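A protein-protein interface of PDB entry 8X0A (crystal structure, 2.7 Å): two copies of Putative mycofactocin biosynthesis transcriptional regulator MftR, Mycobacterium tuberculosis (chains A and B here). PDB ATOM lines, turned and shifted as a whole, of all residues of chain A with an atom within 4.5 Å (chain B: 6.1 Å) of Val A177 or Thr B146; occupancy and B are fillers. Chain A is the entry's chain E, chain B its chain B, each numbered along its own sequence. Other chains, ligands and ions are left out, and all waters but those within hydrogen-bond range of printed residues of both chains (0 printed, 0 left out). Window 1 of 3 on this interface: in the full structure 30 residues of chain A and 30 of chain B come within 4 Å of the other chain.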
ATOM      1  N   THR A 146      11.570  26.020 -10.706  1.00  0.00           N
ATOM      2  CA  THR A 146      11.371  24.584 -10.629  1.00  0.00           C
ATOM      3  C   THR A 146      12.698  23.882 -10.329  1.00  0.00           C
ATOM      4  O   THR A 146      12.779  23.074  -9.429  1.00  0.00           O
ATOM      5  CB  THR A 146      10.741  24.079 -11.926  1.00  0.00           C
ATOM      6  OG1 THR A 146       9.414  24.627 -11.999  1.00  0.00           O
ATOM      7  CG2 THR A 146      10.719  22.565 -12.020  1.00  0.00           C
ATOM      8  N   MET A 147      13.724  24.230 -11.101  1.00  0.00           N
ATOM      9  CA  MET A 147      15.079  23.746 -10.935  1.00  0.00           C
ATOM     10  C   MET A 147      15.621  24.065  -9.536  1.00  0.00           C
ATOM     11  O   MET A 147      16.367  23.264  -8.946  1.00  0.00           O
ATOM     12  CB  MET A 147      16.003  24.402 -11.974  1.00  0.00           C
ATOM     13  CG  MET A 147      16.015  23.915 -13.416  1.00  0.00           C
ATOM     14  SD  MET A 147      16.474  22.212 -13.684  1.00  0.00           S
ATOM     15  CE  MET A 147      14.880  21.517 -13.246  1.00  0.00           C
ATOM     16  N   VAL A 150      13.874  21.670  -7.101  1.00  0.00           N
ATOM     17  CA  VAL A 150      14.503  20.373  -7.285  1.00  0.00           C
ATOM     18  C   VAL A 150      15.796  20.299  -6.456  1.00  0.00           C
ATOM     19  O   VAL A 150      15.964  19.367  -5.673  1.00  0.00           O
ATOM     20  CB  VAL A 150      14.720  20.072  -8.788  1.00  0.00           C
ATOM     21  CG1 VAL A 150      15.779  19.018  -9.049  1.00  0.00           C
ATOM     22  CG2 VAL A 150      13.444  19.581  -9.436  1.00  0.00           C
ATOM     23  N   ALA A 173      15.066  13.904  -7.677  1.00  0.00           N
ATOM     24  CA  ALA A 173      14.279  15.125  -7.583  1.00  0.00           C
ATOM     25  C   ALA A 173      13.991  15.694  -8.981  1.00  0.00           C
ATOM     26  O   ALA A 173      12.875  16.048  -9.276  1.00  0.00           O
ATOM     27  CB  ALA A 173      14.968  16.139  -6.701  1.00  0.00           C
ATOM     28  N   PHE A 174      15.001  15.737  -9.844  1.00  0.00           N
ATOM     29  CA  PHE A 174      14.830  16.146 -11.225  1.00  0.00           C
ATOM     30  C   PHE A 174      13.774  15.316 -11.944  1.00  0.00           C
ATOM     31  O   PHE A 174      12.959  15.854 -12.699  1.00  0.00           O
ATOM     32  CB  PHE A 174      16.159  16.113 -11.992  1.00  0.00           C
ATOM     33  CG  PHE A 174      16.042  16.733 -13.352  1.00  0.00           C
ATOM     34  CD1 PHE A 174      15.568  15.985 -14.419  1.00  0.00           C
ATOM     35  CD2 PHE A 174      16.323  18.075 -13.541  1.00  0.00           C
ATOM     36  CE1 PHE A 174      15.380  16.571 -15.666  1.00  0.00           C
ATOM     37  CE2 PHE A 174      16.100  18.664 -14.784  1.00  0.00           C
ATOM     38  CZ  PHE A 174      15.638  17.919 -15.844  1.00  0.00           C
ATOM     39  N   ASP A 175      13.809  14.009 -11.730  1.00  0.00           N
ATOM     40  CA  ASP A 175      12.987  13.074 -12.506  1.00  0.00           C
ATOM     41  C   ASP A 175      11.502  13.193 -12.178  1.00  0.00           C
ATOM     42  O   ASP A 175      10.675  12.919 -13.044  1.00  0.00           O
ATOM     43  CB  ASP A 175      13.484  11.627 -12.344  1.00  0.00           C
ATOM     44  CG  ASP A 175      14.744  11.318 -13.150  1.00  0.00           C
ATOM     45  OD1 ASP A 175      15.241  12.222 -13.918  1.00  0.00           O
ATOM     46  OD2 ASP A 175      15.238  10.182 -13.010  1.00  0.00           O
ATOM     47  N   VAL A 176      11.170  13.587 -10.937  1.00  0.00           N
ATOM     48  CA  VAL A 176       9.794  13.858 -10.555  1.00  0.00           C
ATOM     49  C   VAL A 176       9.209  14.920 -11.488  1.00  0.00           C
ATOM     50  O   VAL A 176       8.174  14.724 -12.111  1.00  0.00           O
ATOM     51  CB  VAL A 176       9.741  14.297  -9.083  1.00  0.00           C
ATOM     52  CG1 VAL A 176       8.428  15.001  -8.703  1.00  0.00           C
ATOM     53  CG2 VAL A 176      10.024  13.089  -8.195  1.00  0.00           C
ATOM     54  N   VAL A 177       9.943  16.008 -11.581  1.00  0.00           N
ATOM     55  CA  VAL A 177       9.602  17.218 -12.301  1.00  0.00           C
ATOM     56  C   VAL A 177       9.759  17.007 -13.811  1.00  0.00           C
ATOM     57  O   VAL A 177       9.052  17.652 -14.599  1.00  0.00           O
ATOM     58  CB  VAL A 177      10.499  18.346 -11.730  1.00  0.00           C
ATOM     59  CG1 VAL A 177      11.088  19.302 -12.739  1.00  0.00           C
ATOM     60  CG2 VAL A 177       9.785  19.122 -10.645  1.00  0.00           C
ATOM     61  N   GLY A 178      10.733  16.164 -14.217  1.00  0.00           N
ATOM     62  CA  GLY A 178      10.928  15.810 -15.619  1.00  0.00           C
ATOM     63  C   GLY A 178       9.748  15.016 -16.173  1.00  0.00           C
ATOM     64  O   GLY A 178       9.209  15.365 -17.223  1.00  0.00           O
ATOM     65  N   ALA A 179       9.366  13.968 -15.423  1.00  0.00           N
ATOM     66  CA  ALA A 179       8.177  13.159 -15.684  1.00  0.00           C
ATOM     67  C   ALA A 179       6.898  13.988 -15.602  1.00  0.00           C
ATOM     68  O   ALA A 179       6.030  13.839 -16.448  1.00  0.00           O
ATOM     69  CB  ALA A 179       8.114  12.002 -14.711  1.00  0.00           C
ATOM     70  N   GLY A 180       6.803  14.829 -14.560  1.00  0.00           N
ATOM     71  CA  GLY A 180       5.699  15.758 -14.343  1.00  0.00           C
ATOM     72  C   GLY A 180       4.802  15.304 -13.195  1.00  0.00           C
ATOM     73  O   GLY A 180       4.827  14.139 -12.849  1.00  0.00           O
ATOM     74  N   GLN B 141       7.791  16.120  -1.029  1.00  0.00           N
ATOM     75  CA  GLN B 141       8.919  16.916  -0.506  1.00  0.00           C
ATOM     76  C   GLN B 141       9.521  17.654  -1.713  1.00  0.00           C
ATOM     77  O   GLN B 141       9.474  18.882  -1.744  1.00  0.00           O
ATOM     78  CB  GLN B 141       9.987  16.130   0.276  1.00  0.00           C
ATOM     79  CG  GLN B 141      10.850  16.974   1.203  1.00  0.00           C
ATOM     80  CD  GLN B 141      10.111  17.513   2.405  1.00  0.00           C
ATOM     81  OE1 GLN B 141       9.407  16.794   3.105  1.00  0.00           O
ATOM     82  NE2 GLN B 141      10.286  18.793   2.689  1.00  0.00           N
ATOM     83  N   THR B 142       9.899  16.894  -2.762  1.00  0.00           N
ATOM     84  CA  THR B 142      10.138  17.414  -4.103  1.00  0.00           C
ATOM     85  C   THR B 142       8.879  18.073  -4.668  1.00  0.00           C
ATOM     86  O   THR B 142       8.990  19.125  -5.276  1.00  0.00           O
ATOM     87  CB  THR B 142      10.722  16.350  -5.042  1.00  0.00           C
ATOM     88  OG1 THR B 142      11.999  15.952  -4.534  1.00  0.00           O
ATOM     89  CG2 THR B 142      10.984  16.875  -6.438  1.00  0.00           C
ATOM     90  N   VAL B 143       7.711  17.464  -4.471  1.00  0.00           N
ATOM     91  CA  VAL B 143       6.456  18.039  -4.922  1.00  0.00           C
ATOM     92  C   VAL B 143       6.192  19.350  -4.180  1.00  0.00           C
ATOM     93  O   VAL B 143       5.761  20.300  -4.812  1.00  0.00           O
ATOM     94  CB  VAL B 143       5.274  17.051  -4.786  1.00  0.00           C
ATOM     95  CG1 VAL B 143       3.911  17.706  -5.052  1.00  0.00           C
ATOM     96  CG2 VAL B 143       5.457  15.820  -5.675  1.00  0.00           C
ATOM     97  N   ALA B 144       6.457  19.411  -2.866  1.00  0.00           N
ATOM     98  CA  ALA B 144       6.184  20.600  -2.072  1.00  0.00           C
ATOM     99  C   ALA B 144       7.089  21.758  -2.502  1.00  0.00           C
ATOM    100  O   ALA B 144       6.606  22.874  -2.613  1.00  0.00           O
ATOM    101  CB  ALA B 144       6.358  20.292  -0.599  1.00  0.00           C
ATOM    102  N   TRP B 145       8.391  21.483  -2.709  1.00  0.00           N
ATOM    103  CA  TRP B 145       9.380  22.454  -3.170  1.00  0.00           C
ATOM    104  C   TRP B 145       9.078  22.960  -4.575  1.00  0.00           C
ATOM    105  O   TRP B 145       9.275  24.128  -4.889  1.00  0.00           O
ATOM    106  CB  TRP B 145      10.792  21.841  -3.177  1.00  0.00           C
ATOM    107  CG  TRP B 145      11.530  21.953  -1.888  1.00  0.00           C
ATOM    108  CD1 TRP B 145      11.834  20.942  -1.035  1.00  0.00           C
ATOM    109  CD2 TRP B 145      12.100  23.149  -1.323  1.00  0.00           C
ATOM    110  NE1 TRP B 145      12.542  21.423   0.025  1.00  0.00           N
ATOM    111  CE2 TRP B 145      12.723  22.775  -0.113  1.00  0.00           C
ATOM    112  CE3 TRP B 145      12.162  24.497  -1.725  1.00  0.00           C
ATOM    113  CZ2 TRP B 145      13.397  23.695   0.691  1.00  0.00           C
ATOM    114  CZ3 TRP B 145      12.803  25.411  -0.915  1.00  0.00           C
ATOM    115  CH2 TRP B 145      13.412  25.008   0.275  1.00  0.00           C
ATOM    116  N   THR B 146       8.731  22.024  -5.447  1.00  0.00           N
ATOM    117  CA  THR B 146       8.370  22.308  -6.822  1.00  0.00           C
ATOM    118  C   THR B 146       7.172  23.250  -6.841  1.00  0.00           C
ATOM    119  O   THR B 146       7.202  24.252  -7.518  1.00  0.00           O
ATOM    120  CB  THR B 146       8.083  20.994  -7.545  1.00  0.00           C
ATOM    121  OG1 THR B 146       9.337  20.315  -7.696  1.00  0.00           O
ATOM    122  CG2 THR B 146       7.452  21.192  -8.889  1.00  0.00           C
ATOM    123  N   MET B 147       6.145  22.917  -6.072  1.00  0.00           N
ATOM    124  CA  MET B 147       4.953  23.736  -5.933  1.00  0.00           C
ATOM    125  C   MET B 147       5.247  25.111  -5.331  1.00  0.00           C
ATOM    126  O   MET B 147       4.640  26.073  -5.770  1.00  0.00           O
ATOM    127  CB  MET B 147       3.903  22.984  -5.121  1.00  0.00           C
ATOM    128  CG  MET B 147       3.280  21.922  -6.036  1.00  0.00           C
ATOM    129  SD  MET B 147       1.821  21.272  -5.394  1.00  0.00           S
ATOM    130  CE  MET B 147       0.752  22.644  -5.839  1.00  0.00           C
ATOM    131  N   LEU B 148       6.201  25.205  -4.407  1.00  0.00           N
ATOM    132  CA  LEU B 148       6.637  26.491  -3.900  1.00  0.00           C
ATOM    133  C   LEU B 148       7.307  27.320  -5.006  1.00  0.00           C
ATOM    134  O   LEU B 148       7.010  28.510  -5.114  1.00  0.00           O
ATOM    135  CB  LEU B 148       7.583  26.286  -2.708  1.00  0.00           C
ATOM    136  CG  LEU B 148       8.103  27.559  -2.054  1.00  0.00           C
ATOM    137  CD1 LEU B 148       6.951  28.448  -1.571  1.00  0.00           C
ATOM    138  CD2 LEU B 148       9.052  27.156  -0.946  1.00  0.00           C
ATOM    139  N   GLY B 149       8.214  26.714  -5.785  1.00  0.00           N
ATOM    140  CA  GLY B 149       8.838  27.402  -6.908  1.00  0.00           C
ATOM    141  C   GLY B 149       7.835  27.898  -7.964  1.00  0.00           C
ATOM    142  O   GLY B 149       7.938  29.013  -8.460  1.00  0.00           O
ATOM    143  N   VAL B 150       6.866  27.051  -8.317  1.00  0.00           N
ATOM    144  CA  VAL B 150       5.759  27.402  -9.196  1.00  0.00           C
ATOM    145  C   VAL B 150       5.055  28.663  -8.670  1.00  0.00           C
ATOM    146  O   VAL B 150       4.845  29.600  -9.431  1.00  0.00           O
ATOM    147  CB  VAL B 150       4.796  26.190  -9.326  1.00  0.00           C
ATOM    148  CG1 VAL B 150       3.343  26.533  -9.585  1.00  0.00           C
ATOM    149  CG2 VAL B 150       5.286  25.186 -10.345  1.00  0.00           C
ATOM    150  N   ALA B 151       4.701  28.666  -7.370  1.00  0.00           N
ATOM    151  CA  ALA B 151       3.995  29.756  -6.718  1.00  0.00           C
ATOM    152  C   ALA B 151       4.793  31.051  -6.788  1.00  0.00           C
ATOM    153  O   ALA B 151       4.250  32.068  -7.223  1.00  0.00           O
ATOM    154  CB  ALA B 151       3.635  29.391  -5.288  1.00  0.00           C
ATOM    155  N   VAL B 176       3.175  23.679 -16.343  1.00  0.00           N
ATOM    156  CA  VAL B 176       4.501  23.377 -16.868  1.00  0.00           C
ATOM    157  C   VAL B 176       5.040  22.109 -16.192  1.00  0.00           C
ATOM    158  O   VAL B 176       5.399  21.113 -16.839  1.00  0.00           O
ATOM    159  CB  VAL B 176       5.465  24.559 -16.630  1.00  0.00           C
ATOM    160  CG1 VAL B 176       6.921  24.163 -16.897  1.00  0.00           C
ATOM    161  CG2 VAL B 176       5.084  25.814 -17.417  1.00  0.00           C
ATOM    162  N   VAL B 177       5.015  22.187 -14.865  1.00  0.00           N
ATOM    163  CA  VAL B 177       5.560  21.223 -13.937  1.00  0.00           C
ATOM    164  C   VAL B 177       4.654  19.987 -13.861  1.00  0.00           C
ATOM    165  O   VAL B 177       5.152  18.880 -13.592  1.00  0.00           O
ATOM    166  CB  VAL B 177       5.734  21.955 -12.581  1.00  0.00           C
ATOM    167  CG1 VAL B 177       5.320  21.184 -11.350  1.00  0.00           C
ATOM    168  CG2 VAL B 177       7.139  22.471 -12.410  1.00  0.00           C
ATOM    169  N   ALA B 179       2.646  18.851 -16.432  1.00  0.00           N
ATOM    170  CA  ALA B 179       2.940  18.201 -17.706  1.00  0.00           C
ATOM    171  C   ALA B 179       4.325  17.558 -17.662  1.00  0.00           C
ATOM    172  O   ALA B 179       4.480  16.427 -18.118  1.00  0.00           O
ATOM    173  CB  ALA B 179       2.849  19.193 -18.841  1.00  0.00           C
ATOM    174  N   GLY B 180       5.307  18.311 -17.141  1.00  0.00           N
ATOM    175  CA  GLY B 180       6.666  17.854 -16.928  1.00  0.00           C
ATOM    176  C   GLY B 180       7.613  18.503 -17.931  1.00  0.00           C
ATOM    177  O   GLY B 180       7.180  18.971 -18.984  1.00  0.00           O
ATOM    178  N   LEU B 181       8.902  18.527 -17.570  1.00  0.00           N
ATOM    179  CA  LEU B 181       9.944  19.142 -18.385  1.00  0.00           C
ATOM    180  C   LEU B 181      10.237  18.262 -19.599  1.00  0.00           C
ATOM    181  O   LEU B 181      10.618  18.832 -20.625  1.00  0.00           O
ATOM    182  CB  LEU B 181      11.223  19.366 -17.558  1.00  0.00           C
ATOM    183  CG  LEU B 181      11.358  20.650 -16.740  1.00  0.00           C
ATOM    184  CD1 LEU B 181      10.137  20.920 -15.913  1.00  0.00           C
ATOM    185  CD2 LEU B 181      12.575  20.548 -15.856  1.00  0.00           C
ATOM    186  N   ASP B 182      10.001  16.921 -19.498  1.00  0.00           N
ATOM    187  CA  ASP B 182      10.045  15.993 -20.634  1.00  0.00           C
ATOM    188  C   ASP B 182       9.195  16.447 -21.843  1.00  0.00           C
ATOM    189  O   ASP B 182       9.393  15.861 -22.903  1.00  0.00           O
ATOM    190  CB  ASP B 182       9.633  14.561 -20.223  1.00  0.00           C
ATOM    191  CG  ASP B 182      10.699  13.579 -19.748  1.00  0.00           C
ATOM    192  OD1 ASP B 182      11.487  13.147 -20.632  1.00  0.00           O
ATOM    193  OD2 ASP B 182      10.682  13.162 -18.568  1.00  0.00           O
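The backbone carbonyl oxygen (O) of Val A177 is in hydrogen-bond range of the backbone NH (N) of Leu B181, at 3.1 Å. O of Gly A178 is in hydrogen-bond range of N of Leu B181, at 3.2 Å. O of Gly A178 sits at hydrogen-bond distance from N of Asp B182, 2.9 Å away. The backbone carbonyl oxygen (O) of Ala A179 sits close to the backbone carbonyl oxygen (O) of Ala B179 (3.4 Å).
The side-chain hydroxyl (OG1) of Thr B146 lies within hydrogen-bond range of the backbone carbonyl oxygen (O) of Thr B142 (2.7 Å).
Among the printed residues, pairs that only touch across the chains: Thr A146 with Val B177 (3.2 Å), Val A177 with Thr B146 (3.2 Å), Gly A180 with Val B177 (3.3 Å), Val A177 with Gly B180 (3.3 Å), Gly A180 with Gly B180 (3.5 Å), Ala A179 with Asp B182 (3.5 Å), Ala A173 with Thr B142 (3.5 Å), Gly A178 with Gly B180 (3.6 Å), Met A147 with Leu B181 (3.6 Å) and Val A176 with Thr B142 (3.9 Å).
Of the printed residues of chain B, Thr A146 touches Val B177. Printed residues of chain B within 4 Å of Met A147: Leu B181 (3.6 Å). Of the printed residues of chain B, Ala A173 touches Thr B142 (3.5 Å). Of chain B, only Thr B146, Gly B180 and Leu B181 come within 4 Å of Val A177. Printed residues of chain A within 4 Å of Thr B142: Ala A173 (3.5 Å) and Val A176 (3.9 Å). Of chain A, only Val A177 (3.2 Å) comes within 4 Å of Thr B146. Of the printed residues of chain A, Ala B179 touches Ala A179 (3.4 Å). The nearest printed residue of chain A that does not touch Thr B146 is Val A150 (4.5 Å). The nearest printed residue of chain A that does not touch Ala B179 is Gly A180 (4.02 Å).
Of the 17 printed residues of chain B, 7 touch a printed residue of chain A. Printed residues of chain B that touch a printed residue of chain A: Thr B142, Thr B146, Val B177, Ala B179, Gly B180, Leu B181 and Asp B182. Hydrophobic or aromatic side chains of chain B that line the printed part of chain A: Val B177 and Leu B181.
Thr A146 touches Val B177, and with the chains exchanged Val A177 touches Thr B146. Val A177 touches Gly B180, and with the chains exchanged Gly A180 touches Val B177. Ala B179 touches its own counterpart, Ala A179. Gly B180 touches its own counterpart, Gly A180. Of the 14 pairs that touch across the chains among the printed residues, 6 have their exchanged pair printed and touching as well.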
